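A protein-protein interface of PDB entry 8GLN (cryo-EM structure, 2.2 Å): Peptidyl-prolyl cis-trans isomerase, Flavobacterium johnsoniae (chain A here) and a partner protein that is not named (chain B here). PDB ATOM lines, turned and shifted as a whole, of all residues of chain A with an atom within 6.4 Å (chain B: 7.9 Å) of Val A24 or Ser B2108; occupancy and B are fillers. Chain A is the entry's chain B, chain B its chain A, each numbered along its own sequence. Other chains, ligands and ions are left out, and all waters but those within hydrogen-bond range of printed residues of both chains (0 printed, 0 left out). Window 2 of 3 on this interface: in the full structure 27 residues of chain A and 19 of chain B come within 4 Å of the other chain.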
ATOM      1  N   ASP A  22     -33.956 -17.245 -29.135  1.00  0.00           N
ATOM      2  CA  ASP A  22     -33.986 -18.469 -28.344  1.00  0.00           C
ATOM      3  C   ASP A  22     -34.192 -18.173 -26.861  1.00  0.00           C
ATOM      4  O   ASP A  22     -34.005 -17.043 -26.410  1.00  0.00           O
ATOM      5  CB  ASP A  22     -32.696 -19.270 -28.547  1.00  0.00           C
ATOM      6  CG  ASP A  22     -31.447 -18.412 -28.430  1.00  0.00           C
ATOM      7  OD1 ASP A  22     -31.530 -17.296 -27.875  1.00  0.00           O
ATOM      8  OD2 ASP A  22     -30.377 -18.856 -28.897  1.00  0.00           O
ATOM      9  N   GLU A  23     -34.580 -19.201 -26.107  1.00  0.00           N
ATOM     10  CA  GLU A  23     -34.780 -19.066 -24.670  1.00  0.00           C
ATOM     11  C   GLU A  23     -33.946 -20.101 -23.928  1.00  0.00           C
ATOM     12  O   GLU A  23     -34.440 -20.769 -23.014  1.00  0.00           O
ATOM     13  CB  GLU A  23     -36.261 -19.215 -24.305  1.00  0.00           C
ATOM     14  CG  GLU A  23     -37.158 -18.069 -24.762  1.00  0.00           C
ATOM     15  CD  GLU A  23     -37.378 -18.048 -26.264  1.00  0.00           C
ATOM     16  OE1 GLU A  23     -37.231 -19.111 -26.901  1.00  0.00           O
ATOM     17  OE2 GLU A  23     -37.699 -16.969 -26.804  1.00  0.00           O
ATOM     18  N   VAL A  24     -32.679 -20.239 -24.321  1.00  0.00           N
ATOM     19  CA  VAL A  24     -31.803 -21.230 -23.713  1.00  0.00           C
ATOM     20  C   VAL A  24     -31.523 -20.853 -22.265  1.00  0.00           C
ATOM     21  O   VAL A  24     -31.166 -19.709 -21.956  1.00  0.00           O
ATOM     22  CB  VAL A  24     -30.500 -21.354 -24.520  1.00  0.00           C
ATOM     23  CG1 VAL A  24     -29.677 -22.519 -24.015  1.00  0.00           C
ATOM     24  CG2 VAL A  24     -30.810 -21.520 -25.999  1.00  0.00           C
ATOM     25  N   LYS A  25     -31.683 -21.822 -21.365  1.00  0.00           N
ATOM     26  CA  LYS A  25     -31.509 -21.609 -19.935  1.00  0.00           C
ATOM     27  C   LYS A  25     -30.475 -22.587 -19.402  1.00  0.00           C
ATOM     28  O   LYS A  25     -30.462 -23.757 -19.796  1.00  0.00           O
ATOM     29  CB  LYS A  25     -32.833 -21.779 -19.184  1.00  0.00           C
ATOM     30  CG  LYS A  25     -33.943 -20.856 -19.661  1.00  0.00           C
ATOM     31  CD  LYS A  25     -35.319 -21.481 -19.467  1.00  0.00           C
ATOM     32  CE  LYS A  25     -35.293 -22.986 -19.684  1.00  0.00           C
ATOM     33  NZ  LYS A  25     -36.497 -23.649 -19.112  1.00  0.00           N
ATOM     34  N   ASP A  26     -29.618 -22.110 -18.505  1.00  0.00           N
ATOM     35  CA  ASP A  26     -28.582 -22.928 -17.891  1.00  0.00           C
ATOM     36  C   ASP A  26     -29.009 -23.314 -16.481  1.00  0.00           C
ATOM     37  O   ASP A  26     -29.425 -22.456 -15.696  1.00  0.00           O
ATOM     38  CB  ASP A  26     -27.247 -22.183 -17.854  1.00  0.00           C
ATOM     39  CG  ASP A  26     -26.058 -23.120 -17.808  1.00  0.00           C
ATOM     40  OD1 ASP A  26     -26.193 -24.228 -17.250  1.00  0.00           O
ATOM     41  OD2 ASP A  26     -24.986 -22.745 -18.326  1.00  0.00           O
ATOM     42  N   SER A 154     -33.742 -28.812 -20.029  1.00  0.00           N
ATOM     43  CA  SER A 154     -34.135 -27.483 -19.578  1.00  0.00           C
ATOM     44  C   SER A 154     -35.620 -27.212 -19.780  1.00  0.00           C
ATOM     45  O   SER A 154     -36.159 -26.296 -19.150  1.00  0.00           O
ATOM     46  CB  SER A 154     -33.312 -26.421 -20.308  1.00  0.00           C
ATOM     47  OG  SER A 154     -31.937 -26.536 -19.990  1.00  0.00           O
ATOM     48  N   ASN B2099     -30.022 -28.355 -34.001  1.00  0.00           N
ATOM     49  CA  ASN B2099     -29.184 -27.645 -33.041  1.00  0.00           C
ATOM     50  C   ASN B2099     -30.018 -26.746 -32.139  1.00  0.00           C
ATOM     51  O   ASN B2099     -29.773 -26.671 -30.930  1.00  0.00           O
ATOM     52  CB  ASN B2099     -28.115 -26.834 -33.772  1.00  0.00           C
ATOM     53  CG  ASN B2099     -26.953 -27.689 -34.235  1.00  0.00           C
ATOM     54  OD1 ASN B2099     -26.550 -28.629 -33.553  1.00  0.00           O
ATOM     55  ND2 ASN B2099     -26.407 -27.364 -35.399  1.00  0.00           N
ATOM     56  N   ARG B2100     -31.006 -26.052 -32.708  1.00  0.00           N
ATOM     57  CA  ARG B2100     -31.872 -25.207 -31.888  1.00  0.00           C
ATOM     58  C   ARG B2100     -32.657 -26.038 -30.877  1.00  0.00           C
ATOM     59  O   ARG B2100     -32.760 -25.674 -29.698  1.00  0.00           O
ATOM     60  CB  ARG B2100     -32.815 -24.401 -32.779  1.00  0.00           C
ATOM     61  CG  ARG B2100     -32.171 -23.175 -33.400  1.00  0.00           C
ATOM     62  CD  ARG B2100     -33.113 -22.497 -34.373  1.00  0.00           C
ATOM     63  NE  ARG B2100     -34.218 -21.850 -33.679  1.00  0.00           N
ATOM     64  CZ  ARG B2100     -35.411 -21.628 -34.213  1.00  0.00           C
ATOM     65  NH1 ARG B2100     -35.687 -21.979 -35.458  1.00  0.00           N
ATOM     66  NH2 ARG B2100     -36.351 -21.042 -33.478  1.00  0.00           N
ATOM     67  N   ALA B2102     -31.793 -28.972 -29.690  1.00  0.00           N
ATOM     68  CA  ALA B2102     -30.849 -29.488 -28.706  1.00  0.00           C
ATOM     69  C   ALA B2102     -30.488 -28.430 -27.675  1.00  0.00           C
ATOM     70  O   ALA B2102     -30.393 -28.728 -26.480  1.00  0.00           O
ATOM     71  CB  ALA B2102     -29.592 -30.002 -29.404  1.00  0.00           C
ATOM     72  N   GLU B2103     -30.276 -27.188 -28.117  1.00  0.00           N
ATOM     73  CA  GLU B2103     -30.030 -26.110 -27.168  1.00  0.00           C
ATOM     74  C   GLU B2103     -31.233 -25.885 -26.265  1.00  0.00           C
ATOM     75  O   GLU B2103     -31.069 -25.559 -25.085  1.00  0.00           O
ATOM     76  CB  GLU B2103     -29.660 -24.824 -27.906  1.00  0.00           C
ATOM     77  CG  GLU B2103     -28.353 -24.912 -28.672  1.00  0.00           C
ATOM     78  CD  GLU B2103     -27.316 -23.922 -28.177  1.00  0.00           C
ATOM     79  OE1 GLU B2103     -26.120 -24.279 -28.146  1.00  0.00           O
ATOM     80  OE2 GLU B2103     -27.698 -22.787 -27.820  1.00  0.00           O
ATOM     81  N   GLY B2104     -32.444 -26.051 -26.799  1.00  0.00           N
ATOM     82  CA  GLY B2104     -33.623 -26.005 -25.950  1.00  0.00           C
ATOM     83  C   GLY B2104     -33.667 -27.142 -24.946  1.00  0.00           C
ATOM     84  O   GLY B2104     -34.133 -26.968 -23.817  1.00  0.00           O
ATOM     85  N   HIS B2105     -33.182 -28.322 -25.341  1.00  0.00           N
ATOM     86  CA  HIS B2105     -33.210 -29.484 -24.458  1.00  0.00           C
ATOM     87  C   HIS B2105     -31.978 -29.535 -23.563  1.00  0.00           C
ATOM     88  O   HIS B2105     -32.102 -29.696 -22.345  1.00  0.00           O
ATOM     89  CB  HIS B2105     -33.332 -30.766 -25.282  1.00  0.00           C
ATOM     90  CG  HIS B2105     -33.257 -32.018 -24.467  1.00  0.00           C
ATOM     91  ND1 HIS B2105     -32.104 -32.762 -24.349  1.00  0.00           N
ATOM     92  CD2 HIS B2105     -34.195 -32.658 -23.729  1.00  0.00           C
ATOM     93  CE1 HIS B2105     -32.333 -33.806 -23.572  1.00  0.00           C
ATOM     94  NE2 HIS B2105     -33.594 -33.765 -23.183  1.00  0.00           N
ATOM     95  N   TYR B2106     -30.787 -29.406 -24.142  1.00  0.00           N
ATOM     96  CA  TYR B2106     -29.554 -29.220 -23.378  1.00  0.00           C
ATOM     97  C   TYR B2106     -29.277 -27.719 -23.351  1.00  0.00           C
ATOM     98  O   TYR B2106     -28.837 -27.141 -24.348  1.00  0.00           O
ATOM     99  CB  TYR B2106     -28.389 -29.991 -23.991  1.00  0.00           C
ATOM    100  CG  TYR B2106     -28.740 -31.350 -24.560  1.00  0.00           C
ATOM    101  CD1 TYR B2106     -28.672 -32.490 -23.772  1.00  0.00           C
ATOM    102  CD2 TYR B2106     -29.114 -31.495 -25.889  1.00  0.00           C
ATOM    103  CE1 TYR B2106     -28.981 -33.733 -24.287  1.00  0.00           C
ATOM    104  CE2 TYR B2106     -29.426 -32.733 -26.412  1.00  0.00           C
ATOM    105  CZ  TYR B2106     -29.356 -33.849 -25.607  1.00  0.00           C
ATOM    106  OH  TYR B2106     -29.665 -35.085 -26.124  1.00  0.00           O
ATOM    107  N   GLY B2107     -29.526 -27.093 -22.206  1.00  0.00           N
ATOM    108  CA  GLY B2107     -29.526 -25.646 -22.129  1.00  0.00           C
ATOM    109  C   GLY B2107     -28.166 -24.979 -22.081  1.00  0.00           C
ATOM    110  O   GLY B2107     -27.921 -24.130 -21.219  1.00  0.00           O
ATOM    111  N   SER B2108     -27.273 -25.363 -22.994  1.00  0.00           N
ATOM    112  CA  SER B2108     -25.978 -24.714 -23.195  1.00  0.00           C
ATOM    113  C   SER B2108     -25.063 -24.816 -21.980  1.00  0.00           C
ATOM    114  O   SER B2108     -23.945 -24.290 -21.999  1.00  0.00           O
ATOM    115  CB  SER B2108     -26.159 -23.240 -23.578  1.00  0.00           C
ATOM    116  OG  SER B2108     -26.732 -22.490 -22.522  1.00  0.00           O
ATOM    117  N   GLY B2109     -25.516 -25.485 -20.917  1.00  0.00           N
ATOM    118  CA  GLY B2109     -24.667 -25.671 -19.754  1.00  0.00           C
ATOM    119  C   GLY B2109     -23.599 -26.723 -19.930  1.00  0.00           C
ATOM    120  O   GLY B2109     -22.596 -26.699 -19.210  1.00  0.00           O
ATOM    121  N   VAL B2110     -23.794 -27.646 -20.870  1.00  0.00           N
ATOM    122  CA  VAL B2110     -22.827 -28.687 -21.180  1.00  0.00           C
ATOM    123  C   VAL B2110     -22.661 -28.745 -22.691  1.00  0.00           C
ATOM    124  O   VAL B2110     -23.478 -28.220 -23.452  1.00  0.00           O
ATOM    125  CB  VAL B2110     -23.250 -30.071 -20.638  1.00  0.00           C
ATOM    126  CG1 VAL B2110     -23.487 -30.013 -19.137  1.00  0.00           C
ATOM    127  CG2 VAL B2110     -24.495 -30.565 -21.359  1.00  0.00           C
ATOM    128  N   ALA B2111     -21.575 -29.380 -23.123  1.00  0.00           N
ATOM    129  CA  ALA B2111     -21.395 -29.647 -24.541  1.00  0.00           C
ATOM    130  C   ALA B2111     -22.505 -30.565 -25.031  1.00  0.00           C
ATOM    131  O   ALA B2111     -22.818 -31.575 -24.393  1.00  0.00           O
ATOM    132  CB  ALA B2111     -20.026 -30.277 -24.796  1.00  0.00           C
ATOM    133  N   ILE B2112     -23.108 -30.211 -26.160  1.00  0.00           N
ATOM    134  CA  ILE B2112     -24.234 -30.971 -26.693  1.00  0.00           C
ATOM    135  C   ILE B2112     -23.723 -32.329 -27.158  1.00  0.00           C
ATOM    136  O   ILE B2112     -22.825 -32.393 -28.010  1.00  0.00           O
ATOM    137  CB  ILE B2112     -24.932 -30.211 -27.832  1.00  0.00           C
ATOM    138  CG1 ILE B2112     -25.857 -29.133 -27.262  1.00  0.00           C
ATOM    139  CG2 ILE B2112     -25.724 -31.166 -28.712  1.00  0.00           C
ATOM    140  CD1 ILE B2112     -26.135 -28.004 -28.224  1.00  0.00           C
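Of the 13 printed residues of chain B, 6 touch a printed residue of chain A. Printed residues of chain B that touch a printed residue of chain A: Glu B2103, Gly B2104, His B2105, Gly B2107, Ser B2108 and Gly B2109. Along chain A the printed residues that touch a printed residue of chain B span positions 24 to 154.
Among the printed residues, pairs that only touch across the chains: Asp A26 with Gly B2109, Val A24 with Ser B2108, Val A24 with Gly B2107, Val A24 with Glu B2103, Asp A26 with Gly B2107 and Ser A154 with Gly B2104.
Val A24 touches just these residues of chain B: Glu B2103, Gly B2107 and Ser B2108. Printed residues of chain B within 4 Å of Lys A25: Gly B2107. Printed residues of chain B within 4 Å of Asp A26: Gly B2107 and Gly B2109. Printed residues of chain A within 4 Å of Gly B2104: Ser A154 (3.6 Å). Printed residues of chain A within 4 Å of Gly B2107: Val A24 (3.5 Å), Lys A25 (2.9 Å), Asp A26 (3.6 Å) and Ser A154 (3.3 Å). Printed residues of chain A within 4 Å of Ser B2108: Val A24 (3.3 Å). Printed residues of chain A within 4 Å of Gly B2109: Asp A26. The nearest residue of chain B that does not touch Val A24 is Tyr B2106 (4.7 Å). The nearest residue of chain A that does not touch Ser B2108 is Asp A26 (4.1 Å).
The backbone carbonyl oxygen (O) of Ser A154 sits at hydrogen-bond distance from the side-chain amino group (NZ) of Lys A25 (2.7 Å).
O of His B2105 lies within hydrogen-bond range of N of Ser A154. OG of Ser A154 is in hydrogen-bond range of N of Gly B2107. The backbone carbonyl oxygen of Lys A25 lies close to the backbone carbonyl oxygen of Gly B2107, 2.9 Å away.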
